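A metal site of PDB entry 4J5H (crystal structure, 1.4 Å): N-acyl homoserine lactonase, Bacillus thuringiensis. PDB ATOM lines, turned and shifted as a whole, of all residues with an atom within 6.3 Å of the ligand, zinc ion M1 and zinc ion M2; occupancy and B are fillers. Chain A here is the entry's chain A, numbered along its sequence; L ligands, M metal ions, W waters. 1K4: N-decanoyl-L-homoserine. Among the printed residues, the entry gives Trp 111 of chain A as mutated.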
ATOM      1  N   CYS A  18      19.271  11.122   1.672  1.00  0.00           N
ATOM      2  CA  CYS A  18      18.087  10.299   1.593  1.00  0.00           C
ATOM      3  C   CYS A  18      16.900  11.139   1.173  1.00  0.00           C
ATOM      4  O   CYS A  18      16.757  12.286   1.585  1.00  0.00           O
ATOM      5  CB  CYS A  18      17.807   9.552   2.896  1.00  0.00           C
ATOM      6  SG  CYS A  18      17.472  10.591   4.329  1.00  0.00           S
ATOM      7  N   MET A  19      16.060  10.528   0.334  1.00  0.00           N
ATOM      8  CA  MET A  19      14.820  11.146  -0.074  1.00  0.00           C
ATOM      9  C   MET A  19      13.812  10.833   0.991  1.00  0.00           C
ATOM     10  O   MET A  19      13.704   9.693   1.444  1.00  0.00           O
ATOM     11  CB  MET A  19      14.270  10.569  -1.373  1.00  0.00           C
ATOM     12  CG  MET A  19      15.236  10.555  -2.522  1.00  0.00           C
ATOM     13  SD  MET A  19      15.882  12.179  -3.025  1.00  0.00           S
ATOM     14  CE  MET A  19      14.359  13.040  -3.362  1.00  0.00           C
ATOM     15  N   LEU A  20      13.068  11.855   1.381  1.00  0.00           N
ATOM     16  CA  LEU A  20      12.041  11.756   2.393  1.00  0.00           C
ATOM     17  C   LEU A  20      10.837  12.579   1.955  1.00  0.00           C
ATOM     18  O   LEU A  20      10.966  13.733   1.536  1.00  0.00           O
ATOM     19  CB  LEU A  20      12.541  12.284   3.741  1.00  0.00           C
ATOM     20  CG  LEU A  20      11.583  12.226   4.921  1.00  0.00           C
ATOM     21  CD1 LEU A  20      11.118  10.810   5.200  1.00  0.00           C
ATOM     22  CD2 LEU A  20      12.285  12.818   6.148  1.00  0.00           C
ATOM     23  N   LEU A  37      17.470  15.022   1.283  1.00  0.00           N
ATOM     24  CA  LEU A  37      17.979  15.575   2.538  1.00  0.00           C
ATOM     25  C   LEU A  37      19.360  15.061   2.828  1.00  0.00           C
ATOM     26  O   LEU A  37      19.676  13.928   2.454  1.00  0.00           O
ATOM     27  CB  LEU A  37      17.101  15.139   3.693  1.00  0.00           C
ATOM     28  CG  LEU A  37      15.656  15.586   3.669  1.00  0.00           C
ATOM     29  CD1 LEU A  37      14.975  15.030   4.906  1.00  0.00           C
ATOM     30  CD2 LEU A  37      15.591  17.086   3.601  1.00  0.00           C
ATOM     31  N   PHE A  68      13.570   0.137   0.951  1.00  0.00           N
ATOM     32  CA  PHE A  68      12.361   0.054   1.770  1.00  0.00           C
ATOM     33  C   PHE A  68      11.130  -0.371   1.002  1.00  0.00           C
ATOM     34  O   PHE A  68      10.002  -0.291   1.500  1.00  0.00           O
ATOM     35  CB  PHE A  68      12.142   1.360   2.517  1.00  0.00           C
ATOM     36  CG  PHE A  68      13.231   1.642   3.497  1.00  0.00           C
ATOM     37  CD1 PHE A  68      13.559   0.734   4.501  1.00  0.00           C
ATOM     38  CD2 PHE A  68      13.996   2.786   3.367  1.00  0.00           C
ATOM     39  CE1 PHE A  68      14.621   1.001   5.381  1.00  0.00           C
ATOM     40  CE2 PHE A  68      15.039   3.045   4.262  1.00  0.00           C
ATOM     41  CZ  PHE A  68      15.355   2.156   5.248  1.00  0.00           C
ATOM     42  N   THR A  71       7.931  -2.467   2.657  1.00  0.00           N
ATOM     43  CA  THR A  71       7.836  -2.088   4.067  1.00  0.00           C
ATOM     44  C   THR A  71       6.820  -0.975   4.222  1.00  0.00           C
ATOM     45  O   THR A  71       6.336  -0.416   3.221  1.00  0.00           O
ATOM     46  CB  THR A  71       9.169  -1.534   4.611  1.00  0.00           C
ATOM     47  OG1 THR A  71       9.375  -0.201   4.130  1.00  0.00           O
ATOM     48  CG2 THR A  71      10.346  -2.423   4.203  1.00  0.00           C
ATOM     49  N   PHE A  72       6.536  -0.620   5.469  1.00  0.00           N
ATOM     50  CA  PHE A  72       5.542   0.404   5.775  1.00  0.00           C
ATOM     51  C   PHE A  72       5.948   1.822   5.323  1.00  0.00           C
ATOM     52  O   PHE A  72       5.120   2.722   5.331  1.00  0.00           O
ATOM     53  CB  PHE A  72       5.148   0.374   7.273  1.00  0.00           C
ATOM     54  CG  PHE A  72       6.240   0.843   8.214  1.00  0.00           C
ATOM     55  CD1 PHE A  72       7.272  -0.017   8.580  1.00  0.00           C
ATOM     56  CD2 PHE A  72       6.199   2.130   8.754  1.00  0.00           C
ATOM     57  CE1 PHE A  72       8.273   0.425   9.438  1.00  0.00           C
ATOM     58  CE2 PHE A  72       7.206   2.563   9.621  1.00  0.00           C
ATOM     59  CZ  PHE A  72       8.240   1.709   9.958  1.00  0.00           C
ATOM     60  N   VAL A  73       7.209   2.012   4.901  1.00  0.00           N
ATOM     61  CA  VAL A  73       7.668   3.309   4.375  1.00  0.00           C
ATOM     62  C   VAL A  73       8.034   3.285   2.872  1.00  0.00           C
ATOM     63  O   VAL A  73       8.674   4.236   2.378  1.00  0.00           O
ATOM     64  CB  VAL A  73       8.839   3.851   5.205  1.00  0.00           C
ATOM     65  CG1 VAL A  73       8.468   3.910   6.680  1.00  0.00           C
ATOM     66  CG2 VAL A  73      10.088   3.007   5.014  1.00  0.00           C
ATOM     67  N   ILE A  77      10.751   6.874   1.824  1.00  0.00           N
ATOM     68  CA  ILE A  77      12.165   6.983   2.203  1.00  0.00           C
ATOM     69  C   ILE A  77      12.975   6.224   1.166  1.00  0.00           C
ATOM     70  O   ILE A  77      12.761   5.013   0.987  1.00  0.00           O
ATOM     71  CB  ILE A  77      12.448   6.372   3.599  1.00  0.00           C
ATOM     72  CG1 ILE A  77      11.599   7.061   4.678  1.00  0.00           C
ATOM     73  CG2 ILE A  77      13.922   6.475   3.908  1.00  0.00           C
ATOM     74  CD1 ILE A  77      11.839   6.586   6.100  1.00  0.00           C
ATOM     75  N   HIS A 108      20.787   8.362  18.147  1.00  0.00           N
ATOM     76  CA  HIS A 108      19.750   7.423  18.199  1.00  0.00           C
ATOM     77  C   HIS A 108      20.059   6.320  17.181  1.00  0.00           C
ATOM     78  O   HIS A 108      21.063   6.402  16.460  1.00  0.00           O
ATOM     79  CB  HIS A 108      18.385   8.082  18.009  1.00  0.00           C
ATOM     80  CG  HIS A 108      18.120   8.721  16.687  1.00  0.00           C
ATOM     81  ND1 HIS A 108      18.957   9.635  16.070  1.00  0.00           N
ATOM     82  CD2 HIS A 108      17.011   8.666  15.928  1.00  0.00           C
ATOM     83  CE1 HIS A 108      18.361  10.098  14.982  1.00  0.00           C
ATOM     84  NE2 HIS A 108      17.185   9.518  14.875  1.00  0.00           N
ATOM     85  N   HIS A 110      18.043   5.077  14.625  1.00  0.00           N
ATOM     86  CA  HIS A 110      17.451   5.109  13.301  1.00  0.00           C
ATOM     87  C   HIS A 110      18.472   4.782  12.212  1.00  0.00           C
ATOM     88  O   HIS A 110      19.665   4.985  12.393  1.00  0.00           O
ATOM     89  CB  HIS A 110      16.741   6.436  13.030  1.00  0.00           C
ATOM     90  CG  HIS A 110      15.464   6.600  13.796  1.00  0.00           C
ATOM     91  ND1 HIS A 110      14.840   7.818  13.941  1.00  0.00           N
ATOM     92  CD2 HIS A 110      14.686   5.699  14.432  1.00  0.00           C
ATOM     93  CE1 HIS A 110      13.728   7.647  14.649  1.00  0.00           C
ATOM     94  NE2 HIS A 110      13.625   6.378  14.982  1.00  0.00           N
ATOM     95  N   TRP A 111      17.951   4.298  11.096  1.00  0.00           N
ATOM     96  CA  TRP A 111      18.719   3.590  10.073  1.00  0.00           C
ATOM     97  C   TRP A 111      19.846   4.407   9.456  1.00  0.00           C
ATOM     98  O   TRP A 111      20.861   3.864   9.048  1.00  0.00           O
ATOM     99  CB  TRP A 111      17.761   3.019   9.002  1.00  0.00           C
ATOM    100  CG  TRP A 111      17.231   4.096   8.109  1.00  0.00           C
ATOM    101  CD1 TRP A 111      16.229   4.989   8.383  1.00  0.00           C
ATOM    102  CD2 TRP A 111      17.770   4.472   6.852  1.00  0.00           C
ATOM    103  NE1 TRP A 111      16.095   5.886   7.353  1.00  0.00           N
ATOM    104  CE2 TRP A 111      17.026   5.593   6.394  1.00  0.00           C
ATOM    105  CE3 TRP A 111      18.791   3.956   6.037  1.00  0.00           C
ATOM    106  CZ2 TRP A 111      17.285   6.211   5.170  1.00  0.00           C
ATOM    107  CZ3 TRP A 111      19.026   4.575   4.819  1.00  0.00           C
ATOM    108  CH2 TRP A 111      18.285   5.700   4.410  1.00  0.00           C
ATOM    109  N   ASP A 112      19.631   5.710   9.356  1.00  0.00           N
ATOM    110  CA  ASP A 112      20.566   6.636   8.744  1.00  0.00           C
ATOM    111  C   ASP A 112      21.501   7.302   9.749  1.00  0.00           C
ATOM    112  O   ASP A 112      22.310   8.165   9.369  1.00  0.00           O
ATOM    113  CB  ASP A 112      19.875   7.669   7.852  1.00  0.00           C
ATOM    114  CG  ASP A 112      18.860   8.516   8.596  1.00  0.00           C
ATOM    115  OD1 ASP A 112      18.169   8.037   9.515  1.00  0.00           O
ATOM    116  OD2 ASP A 112      18.715   9.686   8.217  1.00  0.00           O
ATOM    117  N   HIS A 113      21.382   6.883  11.002  1.00  0.00           N
ATOM    118  CA  HIS A 113      22.237   7.350  12.097  1.00  0.00           C
ATOM    119  C   HIS A 113      23.113   6.258  12.725  1.00  0.00           C
ATOM    120  O   HIS A 113      24.201   6.565  13.234  1.00  0.00           O
ATOM    121  CB  HIS A 113      21.413   8.007  13.181  1.00  0.00           C
ATOM    122  CG  HIS A 113      20.756   9.237  12.716  1.00  0.00           C
ATOM    123  ND1 HIS A 113      21.332  10.478  12.846  1.00  0.00           N
ATOM    124  CD2 HIS A 113      19.580   9.417  12.081  1.00  0.00           C
ATOM    125  CE1 HIS A 113      20.543  11.365  12.270  1.00  0.00           C
ATOM    126  NE2 HIS A 113      19.463  10.747  11.832  1.00  0.00           N
ATOM    127  N   GLU A 139       9.342  -1.605  15.154  1.00  0.00           N
ATOM    128  CA  GLU A 139       9.449  -1.947  13.731  1.00  0.00           C
ATOM    129  C   GLU A 139      10.294  -0.985  12.899  1.00  0.00           C
ATOM    130  O   GLU A 139      10.754  -1.347  11.835  1.00  0.00           O
ATOM    131  CB  GLU A 139       8.074  -2.080  13.085  1.00  0.00           C
ATOM    132  CG  GLU A 139       7.261  -0.797  13.051  1.00  0.00           C
ATOM    133  CD  GLU A 139       5.812  -1.027  12.600  1.00  0.00           C
ATOM    134  OE1 GLU A 139       5.015  -0.070  12.639  1.00  0.00           O
ATOM    135  OE2 GLU A 139       5.487  -2.174  12.212  1.00  0.00           O
ATOM    136  N   GLU A 140      10.457   0.247  13.371  1.00  0.00           N
ATOM    137  CA  GLU A 140      11.230   1.242  12.622  1.00  0.00           C
ATOM    138  C   GLU A 140      12.753   1.072  12.755  1.00  0.00           C
ATOM    139  O   GLU A 140      13.515   1.910  12.265  1.00  0.00           O
ATOM    140  CB  GLU A 140      10.797   2.678  12.977  1.00  0.00           C
ATOM    141  CG  GLU A 140      11.128   3.175  14.380  1.00  0.00           C
ATOM    142  CD  GLU A 140      10.084   2.867  15.430  1.00  0.00           C
ATOM    143  OE1 GLU A 140      10.119   3.526  16.496  1.00  0.00           O
ATOM    144  OE2 GLU A 140       9.200   1.989  15.207  1.00  0.00           O
ATOM    145  N   TYR A 141      13.193   0.018  13.450  1.00  0.00           N
ATOM    146  CA  TYR A 141      14.624  -0.264  13.603  1.00  0.00           C
ATOM    147  C   TYR A 141      15.094  -1.427  12.754  1.00  0.00           C
ATOM    148  O   TYR A 141      14.482  -2.520  12.771  1.00  0.00           O
ATOM    149  CB  TYR A 141      14.974  -0.510  15.062  1.00  0.00           C
ATOM    150  CG  TYR A 141      14.793   0.770  15.890  1.00  0.00           C
ATOM    151  CD1 TYR A 141      15.815   1.692  15.977  1.00  0.00           C
ATOM    152  CD2 TYR A 141      13.575   1.066  16.508  1.00  0.00           C
ATOM    153  CE1 TYR A 141      15.648   2.841  16.690  1.00  0.00           C
ATOM    154  CE2 TYR A 141      13.401   2.219  17.242  1.00  0.00           C
ATOM    155  CZ  TYR A 141      14.460   3.090  17.352  1.00  0.00           C
ATOM    156  OH  TYR A 141      14.321   4.271  18.036  1.00  0.00           O
ATOM    157  N   MET A 142      16.155  -1.169  11.992  1.00  0.00           N
ATOM    158  CA  MET A 142      16.767  -2.187  11.149  1.00  0.00           C
ATOM    159  C   MET A 142      17.723  -3.015  11.984  1.00  0.00           C
ATOM    160  O   MET A 142      18.355  -2.480  12.900  1.00  0.00           O
ATOM    161  CB  MET A 142      17.549  -1.527  10.001  1.00  0.00           C
ATOM    162  CG  MET A 142      16.718  -0.743   9.002  1.00  0.00           C
ATOM    163  SD  MET A 142      17.675  -0.220   7.583  1.00  0.00           S
ATOM    164  CE  MET A 142      17.974  -1.718   6.670  1.00  0.00           C
ATOM    165  N   HIS A 173      11.373  12.220  19.314  1.00  0.00           N
ATOM    166  CA  HIS A 173      11.535  11.812  17.944  1.00  0.00           C
ATOM    167  C   HIS A 173      11.761  10.295  17.876  1.00  0.00           C
ATOM    168  O   HIS A 173      11.238   9.596  16.973  1.00  0.00           O
ATOM    169  CB  HIS A 173      12.660  12.585  17.258  1.00  0.00           C
ATOM    170  CG  HIS A 173      13.099  11.969  15.982  1.00  0.00           C
ATOM    171  ND1 HIS A 173      12.364  12.027  14.803  1.00  0.00           N
ATOM    172  CD2 HIS A 173      14.179  11.209  15.731  1.00  0.00           C
ATOM    173  CE1 HIS A 173      12.993  11.319  13.883  1.00  0.00           C
ATOM    174  NE2 HIS A 173      14.104  10.839  14.420  1.00  0.00           N
ATOM    175  N   SER A 174      12.614   9.812  18.806  1.00  0.00           N
ATOM    176  CA  SER A 174      12.757   8.393  19.091  1.00  0.00           C
ATOM    177  C   SER A 174      12.774   8.232  20.598  1.00  0.00           C
ATOM    178  O   SER A 174      12.927   9.208  21.314  1.00  0.00           O
ATOM    179  CB  SER A 174      14.022   7.848  18.470  1.00  0.00           C
ATOM    180  OG  SER A 174      15.200   8.322  19.122  1.00  0.00           O
ATOM    181  N   HIS A 177      16.307   9.437  22.037  1.00  0.00           N
ATOM    182  CA  HIS A 177      17.090  10.358  21.258  1.00  0.00           C
ATOM    183  C   HIS A 177      17.910  11.264  22.188  1.00  0.00           C
ATOM    184  O   HIS A 177      17.419  11.713  23.228  1.00  0.00           O
ATOM    185  CB  HIS A 177      16.173  11.208  20.364  1.00  0.00           C
ATOM    186  CG  HIS A 177      16.912  12.109  19.446  1.00  0.00           C
ATOM    187  ND1 HIS A 177      17.404  13.336  19.833  1.00  0.00           N
ATOM    188  CD2 HIS A 177      17.347  11.909  18.187  1.00  0.00           C
ATOM    189  CE1 HIS A 177      18.089  13.859  18.841  1.00  0.00           C
ATOM    190  NE2 HIS A 177      18.065  13.001  17.826  1.00  0.00           N
ATOM    191  N   ILE A 194      20.521  17.250  16.318  1.00  0.00           N
ATOM    192  CA  ILE A 194      20.240  16.016  15.569  1.00  0.00           C
ATOM    193  C   ILE A 194      18.756  15.980  15.258  1.00  0.00           C
ATOM    194  O   ILE A 194      18.219  17.002  14.843  1.00  0.00           O
ATOM    195  CB  ILE A 194      20.822  14.741  16.229  1.00  0.00           C
ATOM    196  CG1 ILE A 194      22.160  15.021  16.919  1.00  0.00           C
ATOM    197  CG2 ILE A 194      20.947  13.632  15.177  1.00  0.00           C
ATOM    198  CD1 ILE A 194      23.309  15.274  15.992  1.00  0.00           C
ATOM    199  N   ASP A 195      18.081  14.860  15.446  1.00  0.00           N
ATOM    200  CA  ASP A 195      16.695  14.738  15.047  1.00  0.00           C
ATOM    201  C   ASP A 195      15.695  15.193  16.133  1.00  0.00           C
ATOM    202  O   ASP A 195      14.501  14.953  15.993  1.00  0.00           O
ATOM    203  CB  ASP A 195      16.379  13.311  14.603  1.00  0.00           C
ATOM    204  CG  ASP A 195      17.020  12.927  13.272  1.00  0.00           C
ATOM    205  OD1 ASP A 195      17.770  13.728  12.716  1.00  0.00           O
ATOM    206  OD2 ASP A 195      16.785  11.788  12.799  1.00  0.00           O
ATOM    207  N   TYR A 198      14.420  18.292  12.727  1.00  0.00           N
ATOM    208  CA  TYR A 198      14.974  18.110  11.398  1.00  0.00           C
ATOM    209  C   TYR A 198      15.392  19.440  10.797  1.00  0.00           C
ATOM    210  O   TYR A 198      16.436  19.542  10.174  1.00  0.00           O
ATOM    211  CB  TYR A 198      13.970  17.452  10.458  1.00  0.00           C
ATOM    212  CG  TYR A 198      13.682  15.989  10.604  1.00  0.00           C
ATOM    213  CD1 TYR A 198      14.438  15.153  11.415  1.00  0.00           C
ATOM    214  CD2 TYR A 198      12.664  15.416   9.866  1.00  0.00           C
ATOM    215  CE1 TYR A 198      14.172  13.800  11.471  1.00  0.00           C
ATOM    216  CE2 TYR A 198      12.385  14.067   9.902  1.00  0.00           C
ATOM    217  CZ  TYR A 198      13.137  13.255  10.707  1.00  0.00           C
ATOM    218  OH  TYR A 198      12.864  11.897  10.751  1.00  0.00           O
ATOM    219  N   ALA A 210       8.106  14.119  11.805  1.00  0.00           N
ATOM    220  CA  ALA A 210       7.985  12.709  12.125  1.00  0.00           C
ATOM    221  C   ALA A 210       8.634  12.382  13.459  1.00  0.00           C
ATOM    222  O   ALA A 210       9.792  12.801  13.736  1.00  0.00           O
ATOM    223  CB  ALA A 210       8.605  11.875  11.042  1.00  0.00           C
ATOM    224  N   GLY A 238      19.021  18.671  12.196  1.00  0.00           N
ATOM    225  CA  GLY A 238      19.348  17.298  11.750  1.00  0.00           C
ATOM    226  C   GLY A 238      19.379  17.010  10.265  1.00  0.00           C
ATOM    227  O   GLY A 238      20.261  16.287   9.763  1.00  0.00           O
ATOM    228  N   HIS A 239      18.407  17.570   9.551  1.00  0.00           N
ATOM    229  CA  HIS A 239      18.253  17.324   8.085  1.00  0.00           C
ATOM    230  C   HIS A 239      17.659  18.562   7.438  1.00  0.00           C
ATOM    231  O   HIS A 239      16.472  18.562   7.027  1.00  0.00           O
ATOM    232  CB  HIS A 239      17.351  16.126   7.805  1.00  0.00           C
ATOM    233  CG  HIS A 239      17.798  14.844   8.445  1.00  0.00           C
ATOM    234  ND1 HIS A 239      18.845  14.097   7.956  1.00  0.00           N
ATOM    235  CD2 HIS A 239      17.335  14.156   9.523  1.00  0.00           C
ATOM    236  CE1 HIS A 239      19.003  13.010   8.688  1.00  0.00           C
ATOM    237  NE2 HIS A 239      18.110  13.030   9.659  1.00  0.00           N
HETATM  238  O   1K4 L   1      15.324   9.561  11.652  1.00  0.00           O
HETATM  239  C   1K4 L   1      15.787   9.691  10.510  1.00  0.00           C
HETATM  240  OXT 1K4 L   1      16.856  10.371  10.330  1.00  0.00           O
HETATM  241  CA  1K4 L   1      15.040   9.035   9.370  1.00  0.00           C
HETATM  242  CB  1K4 L   1      14.845  10.138   8.306  1.00  0.00           C
HETATM  243  CAG 1K4 L   1      14.466   9.632   6.936  1.00  0.00           C
HETATM  244  OAD 1K4 L   1      15.424   8.654   6.521  1.00  0.00           O
HETATM  245  N   1K4 L   1      13.695   8.578   9.754  1.00  0.00           N
HETATM  246  CAQ 1K4 L   1      13.561   7.396  10.360  1.00  0.00           C
HETATM  247  OAB 1K4 L   1      14.493   6.604  10.569  1.00  0.00           O
HETATM  248  CAN 1K4 L   1      12.180   7.021  10.787  1.00  0.00           C
HETATM  249  CAM 1K4 L   1      11.918   5.524  10.721  1.00  0.00           C
HETATM  250  CAL 1K4 L   1      11.968   5.053   9.278  1.00  0.00           C
HETATM  251  CAK 1K4 L   1      11.529   3.602   9.127  1.00  0.00           C
HETATM  252  CAJ 1K4 L   1      12.654   2.696   8.678  1.00  0.00           C
HETATM  253  CAI 1K4 L   1      12.068   1.329   8.306  1.00  0.00           C
HETATM  254  CAH 1K4 L   1      12.871   0.192   8.935  1.00  0.00           C
HETATM  255  CAF 1K4 L   1      12.710  -1.159   8.220  1.00  0.00           C
HETATM  256  CAA 1K4 L   1      11.280  -1.496   7.869  1.00  0.00           C
HETATM  257 ZN    ZN M   1      17.806  11.662  11.120  1.00  0.00          ZN
HETATM  258 ZN    ZN M   2      15.622   9.785  13.511  1.00  0.00          ZN
HETATM  259  O   HOH W   1      15.067   3.912  11.456  1.00  0.00           O
HETATM  260  O   HOH W   2      11.028  10.387   9.016  1.00  0.00           O
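OAD of the ligand lies within hydrogen-bond range of NE1 of Trp 111.
OAD of the ligand sits at hydrogen-bond distance from SG of Cys 18, 3.6 Å away.
The backbone NH (N) of Asp 195 lies within hydrogen-bond range of a ring nitrogen (NE2) of His 177 (3.0 Å).
The backbone carbonyl oxygen (O) of Tyr 198 is in hydrogen-bond range of the backbone NH (N) of His 239, at 2.9 Å.
A ring nitrogen (ND1) of His 173 is in hydrogen-bond range of the backbone carbonyl oxygen of Ala 210, 2.9 Å away.
N of Gly 238 lies within hydrogen-bond range of O of Tyr 198 (3.4 Å).
The backbone carbonyl oxygen (O) of Cys 18 lies within hydrogen-bond range of the backbone NH (N) of Leu 37 (2.8 Å).
OG1 of Thr 71 sits at hydrogen-bond distance from O of Phe 68, 2.7 Å away.
The side-chain hydroxyl (OG1) of Thr 71 lies close to the backbone NH (N) of Val 73.
An oxygen (OXT) of the ligand sits close to the side-chain carboxylate of Asp 112, 2.8 Å away.
Merely in contact with the ligand: Tyr 198 (3.5 Å), Ile 77 (3.5 Å), Glu 140 (3.8 Å), Thr 71 (3.9 Å), Phe 72 (3.9 Å), Phe 68 (3.9 Å), Glu 139 (3.9 Å), Val 73 (3.9 Å), Leu 20 (3.9 Å) and Met 142 (3.96 Å).
Hydrophobic or aromatic side chains that line the ligand: Leu 20, Phe 68, Phe 72, Val 73, Ile 77, His 110, Trp 111, His 113, Met 142, His 173 and His 239.
19 residues have an atom within 4 Å of the ligand: Cys 18, Leu 20, Phe 68, Thr 71, Phe 72, Val 73, Ile 77, His 108, His 110, Trp 111, Asp 112, His 113, Glu 139, Glu 140, Met 142, His 173, Asp 195, Tyr 198 and His 239.
Asp 112 touches zinc ion M1 (OD2 to ZN, 3.6 Å).
The nearest printed residue that does not touch zinc ion M2 is His 113 (4.2 Å).
Zinc ion M1 is bound by OXT of the ligand (1.8 Å), OD2 of Asp 195 (2.0 Å), NE2 of His 113 (2.0 Å) and NE2 of His 239 (2.0 Å).
Zinc ion M1 has four donor atoms within binding distance.
Slightly farther from zinc ion M1 lies OD1 of Asp 195 (2.6 Å).
Zinc ion M2 is bound by an oxygen (O) of the ligand (1.9 Å), a ring nitrogen (NE2) of His 173 (2.1 Å), a ring nitrogen (NE2) of His 108 (2.1 Å), a ring nitrogen (ND1) of His 110 (2.2 Å) and the side-chain carboxylate (OD2) of Asp 195 (2.4 Å).
Water W1 lies within hydrogen-bond range of the backbone carbonyl oxygen (O) of Glu 140, an oxygen (OAB) of the ligand and the backbone NH (N) of Trp 111.
Water W2 bridges the side-chain hydroxyl of Tyr 198 (2.9 Å) and a nitrogen (N) of the ligand (3.3 Å).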
